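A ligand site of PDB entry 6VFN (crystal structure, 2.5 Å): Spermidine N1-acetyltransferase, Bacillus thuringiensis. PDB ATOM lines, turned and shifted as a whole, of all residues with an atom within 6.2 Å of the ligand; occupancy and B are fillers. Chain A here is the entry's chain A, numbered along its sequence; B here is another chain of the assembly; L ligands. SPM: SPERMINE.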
ATOM      1  N   HIS A  49     -19.672   5.415 -23.428  1.00  0.00           N
ATOM      2  CA  HIS A  49     -19.782   4.480 -22.316  1.00  0.00           C
ATOM      3  C   HIS A  49     -19.714   3.020 -22.758  1.00  0.00           C
ATOM      4  O   HIS A  49     -20.104   2.125 -21.999  1.00  0.00           O
ATOM      5  CB  HIS A  49     -21.061   4.734 -21.513  1.00  0.00           C
ATOM      6  CG  HIS A  49     -21.055   6.062 -20.807  1.00  0.00           C
ATOM      7  ND1 HIS A  49     -20.575   6.220 -19.528  1.00  0.00           N
ATOM      8  CD2 HIS A  49     -21.446   7.290 -21.220  1.00  0.00           C
ATOM      9  CE1 HIS A  49     -20.673   7.493 -19.174  1.00  0.00           C
ATOM     10  NE2 HIS A  49     -21.197   8.160 -20.183  1.00  0.00           N
ATOM     11  N   ILE A  50     -19.227   2.759 -23.976  1.00  0.00           N
ATOM     12  CA  ILE A  50     -19.078   1.381 -24.457  1.00  0.00           C
ATOM     13  C   ILE A  50     -18.214   0.577 -23.502  1.00  0.00           C
ATOM     14  O   ILE A  50     -18.554  -0.554 -23.118  1.00  0.00           O
ATOM     15  CB  ILE A  50     -18.503   1.378 -25.879  1.00  0.00           C
ATOM     16  CG1 ILE A  50     -19.571   1.748 -26.911  1.00  0.00           C
ATOM     17  CG2 ILE A  50     -17.900   0.018 -26.217  1.00  0.00           C
ATOM     18  CD1 ILE A  50     -19.010   2.015 -28.286  1.00  0.00           C
ATOM     19  N   HIS A  51     -17.075   1.135 -23.101  1.00  0.00           N
ATOM     20  CA  HIS A  51     -16.126   0.464 -22.213  1.00  0.00           C
ATOM     21  C   HIS A  51     -16.212   0.973 -20.780  1.00  0.00           C
ATOM     22  O   HIS A  51     -15.289   0.745 -19.991  1.00  0.00           O
ATOM     23  CB  HIS A  51     -14.710   0.611 -22.760  1.00  0.00           C
ATOM     24  CG  HIS A  51     -14.528   0.029 -24.129  1.00  0.00           C
ATOM     25  ND1 HIS A  51     -14.632  -1.323 -24.374  1.00  0.00           N
ATOM     26  CD2 HIS A  51     -14.274   0.621 -25.319  1.00  0.00           C
ATOM     27  CE1 HIS A  51     -14.439  -1.546 -25.657  1.00  0.00           C
ATOM     28  NE2 HIS A  51     -14.216  -0.387 -26.254  1.00  0.00           N
ATOM     29  N   ASP A  52     -17.293   1.657 -20.427  1.00  0.00           N
ATOM     30  CA  ASP A  52     -17.540   2.063 -19.060  1.00  0.00           C
ATOM     31  C   ASP A  52     -18.037   0.845 -18.284  1.00  0.00           C
ATOM     32  O   ASP A  52     -19.173   0.399 -18.475  1.00  0.00           O
ATOM     33  CB  ASP A  52     -18.552   3.204 -19.009  1.00  0.00           C
ATOM     34  CG  ASP A  52     -18.814   3.704 -17.603  1.00  0.00           C
ATOM     35  OD1 ASP A  52     -18.111   3.270 -16.662  1.00  0.00           O
ATOM     36  OD2 ASP A  52     -19.721   4.549 -17.433  1.00  0.00           O
ATOM     37  N   GLN A  53     -17.193   0.305 -17.399  1.00  0.00           N
ATOM     38  CA  GLN A  53     -17.565  -0.889 -16.657  1.00  0.00           C
ATOM     39  C   GLN A  53     -18.455  -0.581 -15.460  1.00  0.00           C
ATOM     40  O   GLN A  53     -18.971  -1.519 -14.841  1.00  0.00           O
ATOM     41  CB  GLN A  53     -16.309  -1.625 -16.185  1.00  0.00           C
ATOM     42  CG  GLN A  53     -15.284  -1.841 -17.293  1.00  0.00           C
ATOM     43  CD  GLN A  53     -15.845  -2.603 -18.483  1.00  0.00           C
ATOM     44  OE1 GLN A  53     -16.665  -3.504 -18.329  1.00  0.00           O
ATOM     45  NE2 GLN A  53     -15.405  -2.232 -19.673  1.00  0.00           N
ATOM     46  N   SER A  54     -18.658   0.696 -15.128  1.00  0.00           N
ATOM     47  CA  SER A  54     -19.616   1.093 -14.096  1.00  0.00           C
ATOM     48  C   SER A  54     -21.066   0.896 -14.520  1.00  0.00           C
ATOM     49  O   SER A  54     -21.960   1.139 -13.708  1.00  0.00           O
ATOM     50  CB  SER A  54     -19.381   2.552 -13.705  1.00  0.00           C
ATOM     51  OG  SER A  54     -19.852   3.428 -14.719  1.00  0.00           O
ATOM     52  N   GLU A  55     -21.308   0.479 -15.763  1.00  0.00           N
ATOM     53  CA  GLU A  55     -22.651   0.423 -16.321  1.00  0.00           C
ATOM     54  C   GLU A  55     -22.911  -0.947 -16.923  1.00  0.00           C
ATOM     55  O   GLU A  55     -22.013  -1.586 -17.471  1.00  0.00           O
ATOM     56  CB  GLU A  55     -22.850   1.489 -17.398  1.00  0.00           C
ATOM     57  CG  GLU A  55     -23.753   2.646 -17.018  1.00  0.00           C
ATOM     58  CD  GLU A  55     -24.045   3.538 -18.202  1.00  0.00           C
ATOM     59  OE1 GLU A  55     -24.737   4.569 -18.022  1.00  0.00           O
ATOM     60  OE2 GLU A  55     -23.570   3.212 -19.312  1.00  0.00           O
ATOM     61  N   ARG A  56     -24.172  -1.388 -16.827  1.00  0.00           N
ATOM     62  CA  ARG A  56     -24.655  -2.558 -17.551  1.00  0.00           C
ATOM     63  C   ARG A  56     -26.028  -2.191 -18.105  1.00  0.00           C
ATOM     64  O   ARG A  56     -27.011  -2.130 -17.347  1.00  0.00           O
ATOM     65  CB  ARG A  56     -24.723  -3.792 -16.663  1.00  0.00           C
ATOM     66  CG  ARG A  56     -23.370  -4.343 -16.237  1.00  0.00           C
ATOM     67  CD  ARG A  56     -22.523  -4.740 -17.439  1.00  0.00           C
ATOM     68  NE  ARG A  56     -21.284  -5.392 -17.052  1.00  0.00           N
ATOM     69  CZ  ARG A  56     -20.195  -4.760 -16.629  1.00  0.00           C
ATOM     70  NH1 ARG A  56     -20.183  -3.430 -16.537  1.00  0.00           N
ATOM     71  NH2 ARG A  56     -19.104  -5.440 -16.292  1.00  0.00           N
ATOM     72  N   ARG A  57     -26.091  -1.935 -19.409  1.00  0.00           N
ATOM     73  CA  ARG A  57     -27.332  -1.556 -20.070  1.00  0.00           C
ATOM     74  C   ARG A  57     -27.906  -2.774 -20.791  1.00  0.00           C
ATOM     75  O   ARG A  57     -27.200  -3.411 -21.589  1.00  0.00           O
ATOM     76  CB  ARG A  57     -27.071  -0.406 -21.060  1.00  0.00           C
ATOM     77  CG  ARG A  57     -26.529   0.853 -20.394  1.00  0.00           C
ATOM     78  CD  ARG A  57     -26.529   2.046 -21.346  1.00  0.00           C
ATOM     79  NE  ARG A  57     -27.830   2.690 -21.457  1.00  0.00           N
ATOM     80  CZ  ARG A  57     -28.084   3.713 -22.265  1.00  0.00           C
ATOM     81  NH1 ARG A  57     -27.112   4.204 -23.019  1.00  0.00           N
ATOM     82  NH2 ARG A  57     -29.297   4.239 -22.305  1.00  0.00           N
ATOM     83  N   ASN B  22     -20.647 -14.806 -26.559  1.00  0.00           N
ATOM     84  CA  ASN B  22     -20.190 -14.016 -25.428  1.00  0.00           C
ATOM     85  C   ASN B  22     -21.314 -13.529 -24.516  1.00  0.00           C
ATOM     86  O   ASN B  22     -21.032 -13.022 -23.431  1.00  0.00           O
ATOM     87  CB  ASN B  22     -19.382 -12.809 -25.918  1.00  0.00           C
ATOM     88  CG  ASN B  22     -17.966 -13.187 -26.325  1.00  0.00           C
ATOM     89  OD1 ASN B  22     -17.595 -14.361 -26.294  1.00  0.00           O
ATOM     90  ND2 ASN B  22     -17.166 -12.189 -26.693  1.00  0.00           N
ATOM     91  N   MET B  28     -20.518 -18.743 -21.420  1.00  0.00           N
ATOM     92  CA  MET B  28     -19.580 -17.875 -20.711  1.00  0.00           C
ATOM     93  C   MET B  28     -19.382 -18.272 -19.274  1.00  0.00           C
ATOM     94  O   MET B  28     -18.811 -17.475 -18.520  1.00  0.00           O
ATOM     95  CB  MET B  28     -20.055 -16.408 -20.771  1.00  0.00           C
ATOM     96  CG  MET B  28     -19.932 -15.761 -22.133  1.00  0.00           C
ATOM     97  SD  MET B  28     -18.225 -15.654 -22.719  1.00  0.00           S
ATOM     98  CE  MET B  28     -18.228 -16.894 -23.999  1.00  0.00           C
ATOM     99  N   TRP B  31     -15.579 -20.832 -19.767  1.00  0.00           N
ATOM    100  CA  TRP B  31     -14.688 -19.723 -19.519  1.00  0.00           C
ATOM    101  C   TRP B  31     -15.308 -18.891 -18.417  1.00  0.00           C
ATOM    102  O   TRP B  31     -16.526 -18.745 -18.330  1.00  0.00           O
ATOM    103  CB  TRP B  31     -14.477 -18.872 -20.773  1.00  0.00           C
ATOM    104  CG  TRP B  31     -14.019 -19.587 -22.018  1.00  0.00           C
ATOM    105  CD1 TRP B  31     -13.833 -20.923 -22.205  1.00  0.00           C
ATOM    106  CD2 TRP B  31     -13.659 -18.960 -23.248  1.00  0.00           C
ATOM    107  NE1 TRP B  31     -13.398 -21.170 -23.482  1.00  0.00           N
ATOM    108  CE2 TRP B  31     -13.287 -19.980 -24.144  1.00  0.00           C
ATOM    109  CE3 TRP B  31     -13.635 -17.636 -23.686  1.00  0.00           C
ATOM    110  CZ2 TRP B  31     -12.884 -19.712 -25.456  1.00  0.00           C
ATOM    111  CZ3 TRP B  31     -13.228 -17.374 -24.975  1.00  0.00           C
ATOM    112  CH2 TRP B  31     -12.862 -18.402 -25.838  1.00  0.00           C
ATOM    113  N   GLU B  33     -15.973 -15.832 -17.625  1.00  0.00           N
ATOM    114  CA  GLU B  33     -16.160 -14.489 -18.149  1.00  0.00           C
ATOM    115  C   GLU B  33     -17.576 -14.027 -17.860  1.00  0.00           C
ATOM    116  O   GLU B  33     -18.532 -14.809 -17.923  1.00  0.00           O
ATOM    117  CB  GLU B  33     -15.908 -14.456 -19.666  1.00  0.00           C
ATOM    118  CG  GLU B  33     -14.543 -14.969 -20.072  1.00  0.00           C
ATOM    119  CD  GLU B  33     -13.517 -13.862 -20.151  1.00  0.00           C
ATOM    120  OE1 GLU B  33     -13.817 -12.800 -20.729  1.00  0.00           O
ATOM    121  OE2 GLU B  33     -12.390 -14.060 -19.646  1.00  0.00           O
ATOM    122  N   GLU B  34     -17.715 -12.748 -17.535  1.00  0.00           N
ATOM    123  CA  GLU B  34     -19.039 -12.164 -17.388  1.00  0.00           C
ATOM    124  C   GLU B  34     -19.767 -12.224 -18.727  1.00  0.00           C
ATOM    125  O   GLU B  34     -19.223 -11.770 -19.752  1.00  0.00           O
ATOM    126  CB  GLU B  34     -18.934 -10.724 -16.896  1.00  0.00           C
ATOM    127  CG  GLU B  34     -20.068  -9.832 -17.345  1.00  0.00           C
ATOM    128  CD  GLU B  34     -20.039  -8.473 -16.682  1.00  0.00           C
ATOM    129  OE1 GLU B  34     -21.122  -7.890 -16.475  1.00  0.00           O
ATOM    130  OE2 GLU B  34     -18.925  -7.989 -16.377  1.00  0.00           O
ATOM    131  N   PRO B  35     -20.988 -12.771 -18.777  1.00  0.00           N
ATOM    132  CA  PRO B  35     -21.719 -12.917 -20.042  1.00  0.00           C
ATOM    133  C   PRO B  35     -22.402 -11.637 -20.516  1.00  0.00           C
ATOM    134  O   PRO B  35     -23.603 -11.599 -20.779  1.00  0.00           O
ATOM    135  CB  PRO B  35     -22.739 -14.012 -19.706  1.00  0.00           C
ATOM    136  CG  PRO B  35     -23.007 -13.833 -18.254  1.00  0.00           C
ATOM    137  CD  PRO B  35     -21.708 -13.374 -17.639  1.00  0.00           C
ATOM    138  N   TYR B  36     -21.619 -10.554 -20.619  1.00  0.00           N
ATOM    139  CA  TYR B  36     -22.102  -9.291 -21.148  1.00  0.00           C
ATOM    140  C   TYR B  36     -21.036  -8.733 -22.081  1.00  0.00           C
ATOM    141  O   TYR B  36     -19.892  -8.537 -21.679  1.00  0.00           O
ATOM    142  CB  TYR B  36     -22.395  -8.280 -20.036  1.00  0.00           C
ATOM    143  CG  TYR B  36     -23.007  -6.978 -20.516  1.00  0.00           C
ATOM    144  CD1 TYR B  36     -24.381  -6.768 -20.434  1.00  0.00           C
ATOM    145  CD2 TYR B  36     -22.224  -5.975 -21.061  1.00  0.00           C
ATOM    146  CE1 TYR B  36     -24.944  -5.589 -20.864  1.00  0.00           C
ATOM    147  CE2 TYR B  36     -22.788  -4.785 -21.501  1.00  0.00           C
ATOM    148  CZ  TYR B  36     -24.148  -4.605 -21.399  1.00  0.00           C
ATOM    149  OH  TYR B  36     -24.718  -3.423 -21.836  1.00  0.00           O
ATOM    150  N   GLU B  37     -21.432  -8.447 -23.320  1.00  0.00           N
ATOM    151  CA  GLU B  37     -20.572  -7.728 -24.242  1.00  0.00           C
ATOM    152  C   GLU B  37     -21.449  -7.200 -25.370  1.00  0.00           C
ATOM    153  O   GLU B  37     -21.967  -7.986 -26.161  1.00  0.00           O
ATOM    154  CB  GLU B  37     -19.465  -8.616 -24.780  1.00  0.00           C
ATOM    155  CG  GLU B  37     -18.366  -7.847 -25.498  1.00  0.00           C
ATOM    156  CD  GLU B  37     -17.125  -8.675 -25.715  1.00  0.00           C
ATOM    157  OE1 GLU B  37     -17.255  -9.823 -26.186  1.00  0.00           O
ATOM    158  OE2 GLU B  37     -16.022  -8.183 -25.409  1.00  0.00           O
ATOM    159  N   ALA B  38     -21.620  -5.882 -25.422  1.00  0.00           N
ATOM    160  CA  ALA B  38     -22.263  -5.283 -26.589  1.00  0.00           C
ATOM    161  C   ALA B  38     -21.442  -5.586 -27.832  1.00  0.00           C
ATOM    162  O   ALA B  38     -20.219  -5.741 -27.776  1.00  0.00           O
ATOM    163  CB  ALA B  38     -22.412  -3.771 -26.389  1.00  0.00           C
ATOM    164  N   GLU B  41     -18.816  -3.218 -28.409  1.00  0.00           N
ATOM    165  CA  GLU B  41     -17.726  -3.409 -27.450  1.00  0.00           C
ATOM    166  C   GLU B  41     -16.795  -4.526 -27.906  1.00  0.00           C
ATOM    167  O   GLU B  41     -15.567  -4.375 -27.870  1.00  0.00           O
ATOM    168  CB  GLU B  41     -18.295  -3.720 -26.069  1.00  0.00           C
ATOM    169  CG  GLU B  41     -17.238  -4.161 -25.069  1.00  0.00           C
ATOM    170  CD  GLU B  41     -17.809  -4.462 -23.697  1.00  0.00           C
ATOM    171  OE1 GLU B  41     -19.047  -4.552 -23.576  1.00  0.00           O
ATOM    172  OE2 GLU B  41     -17.020  -4.637 -22.744  1.00  0.00           O
ATOM    173  N   LEU B  42     -17.367  -5.658 -28.322  1.00  0.00           N
ATOM    174  CA  LEU B  42     -16.555  -6.756 -28.824  1.00  0.00           C
ATOM    175  C   LEU B  42     -15.774  -6.337 -30.070  1.00  0.00           C
ATOM    176  O   LEU B  42     -14.590  -6.664 -30.208  1.00  0.00           O
ATOM    177  CB  LEU B  42     -17.443  -7.963 -29.144  1.00  0.00           C
ATOM    178  CG  LEU B  42     -16.849  -9.066 -30.023  1.00  0.00           C
ATOM    179  CD1 LEU B  42     -15.841  -9.888 -29.229  1.00  0.00           C
ATOM    180  CD2 LEU B  42     -17.952  -9.956 -30.578  1.00  0.00           C
ATOM    181  N   LEU B  45     -12.863  -4.052 -28.936  1.00  0.00           N
ATOM    182  CA  LEU B  45     -11.797  -4.829 -28.308  1.00  0.00           C
ATOM    183  C   LEU B  45     -11.025  -5.640 -29.337  1.00  0.00           C
ATOM    184  O   LEU B  45      -9.787  -5.730 -29.285  1.00  0.00           O
ATOM    185  CB  LEU B  45     -12.381  -5.730 -27.221  1.00  0.00           C
ATOM    186  CG  LEU B  45     -12.931  -5.006 -25.995  1.00  0.00           C
ATOM    187  CD1 LEU B  45     -13.521  -5.993 -24.997  1.00  0.00           C
ATOM    188  CD2 LEU B  45     -11.850  -4.149 -25.337  1.00  0.00           C
ATOM    189  N   ARG B  57      -6.645 -15.936 -31.861  1.00  0.00           N
ATOM    190  CA  ARG B  57      -8.076 -16.202 -31.846  1.00  0.00           C
ATOM    191  C   ARG B  57      -8.457 -16.959 -33.107  1.00  0.00           C
ATOM    192  O   ARG B  57      -8.144 -16.512 -34.221  1.00  0.00           O
ATOM    193  CB  ARG B  57      -8.864 -14.890 -31.739  1.00  0.00           C
ATOM    194  CG  ARG B  57      -8.566 -14.090 -30.464  1.00  0.00           C
ATOM    195  CD  ARG B  57      -9.534 -12.931 -30.256  1.00  0.00           C
ATOM    196  NE  ARG B  57     -10.803 -13.338 -29.653  1.00  0.00           N
ATOM    197  CZ  ARG B  57     -11.813 -12.501 -29.436  1.00  0.00           C
ATOM    198  NH1 ARG B  57     -11.711 -11.216 -29.762  1.00  0.00           N
ATOM    199  NH2 ARG B  57     -12.935 -12.949 -28.884  1.00  0.00           N
HETATM  200  N1  SPM L   1     -15.417 -13.370 -23.479  1.00  0.00           N
HETATM  201  C2  SPM L   1     -16.354 -12.261 -23.369  1.00  0.00           C
HETATM  202  C3  SPM L   1     -15.621 -10.940 -23.566  1.00  0.00           C
HETATM  203  C4  SPM L   1     -15.167 -10.367 -22.230  1.00  0.00           C
HETATM  204  N5  SPM L   1     -16.246  -9.702 -21.507  1.00  0.00           N
HETATM  205  C6  SPM L   1     -15.969  -9.137 -20.198  1.00  0.00           C
HETATM  206  C7  SPM L   1     -17.134  -8.324 -19.658  1.00  0.00           C
HETATM  207  C8  SPM L   1     -17.110  -6.902 -20.211  1.00  0.00           C
HETATM  208  C9  SPM L   1     -18.341  -6.125 -19.782  1.00  0.00           C
HETATM  209  N10 SPM L   1     -18.360  -4.783 -20.319  1.00  0.00           N
HETATM  210  C11 SPM L   1     -19.504  -3.923 -20.042  1.00  0.00           C
HETATM  211  C12 SPM L   1     -19.329  -2.525 -20.629  1.00  0.00           C
HETATM  212  C13 SPM L   1     -20.604  -1.717 -20.459  1.00  0.00           C
HETATM  213  N14 SPM L   1     -20.399  -0.374 -20.994  1.00  0.00           N
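The backbone carbonyl oxygen of His 49 lies within hydrogen-bond range of a nitrogen (N14) of the ligand (2.7 Å). The side-chain carboxylate (OE2) of Glu 41 of chain B is in salt-bridge range of a nitrogen (N10) of the ligand (2.8 Å). O of Ile 50 lies within hydrogen-bond range of N14 of the ligand, at 2.8 Å. O of Asp 52 is in hydrogen-bond range of N14 of the ligand (2.9 Å). A nitrogen (N10) of the ligand sits at hydrogen-bond distance from the side-chain amide oxygen of Gln 53. The side-chain carboxylate (OE1) of Glu 33 of chain B is in salt-bridge range of a nitrogen (N1) of the ligand. N1 of the ligand sits at hydrogen-bond distance from SD of Met 28 of chain B, at 3.7 Å.
O of Glu 55 touches C13 of the ligand, 3.3 Å away. CZ of Arg 56 touches C11 of the ligand, 3.6 Å away. Asn 22 of chain B touches the ligand (ND2 to C2, 3.4 Å). Glu 34 of chain B touches the ligand (OE2 to C7, 3.8 Å). Tyr 36 of chain B touches the ligand. Glu 37 of chain B touches the ligand. 13 residues have an atom within 4 Å of the ligand: His 49, Ile 50, Asp 52, Gln 53, Glu 55, Arg 56, Asn 22 of chain B, Met 28 of chain B, Glu 33 of chain B, Glu 34 of chain B, Tyr 36 of chain B, Glu 37 of chain B and Glu 41 of chain B. Along chain A the residues within 4 Å of the ligand span positions 49 to 56.
OD2 of Asp 52 is in hydrogen-bond range of ND1 of His 49, at 2.8 Å. The side-chain carboxylate (OE1) of Glu 41 of chain B sits at hydrogen-bond distance from the backbone NH (N) of Ala 38 of chain B (3.4 Å). OG of Ser 54 lies within hydrogen-bond range of OD1 of Asp 52. The guanidinium group of Arg 56 is in hydrogen-bond range of the backbone carbonyl oxygen of Gln 53 (2.8 Å). The side-chain amide nitrogen (NE2) of Gln 53 is in hydrogen-bond range of the backbone carbonyl oxygen (O) of His 51 (3.0 Å). The backbone carbonyl oxygen of Met 28 of chain B sits at hydrogen-bond distance from the backbone NH of Glu 33 of chain B (3.4 Å). The side-chain hydroxyl (OH) of Tyr 36 of chain B lies within hydrogen-bond range of the backbone carbonyl oxygen (O) of Arg 57 of chain A (2.5 Å). NH2 of Arg 56 is in salt-bridge range of OE2 of Glu 34 of chain B (2.6 Å).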
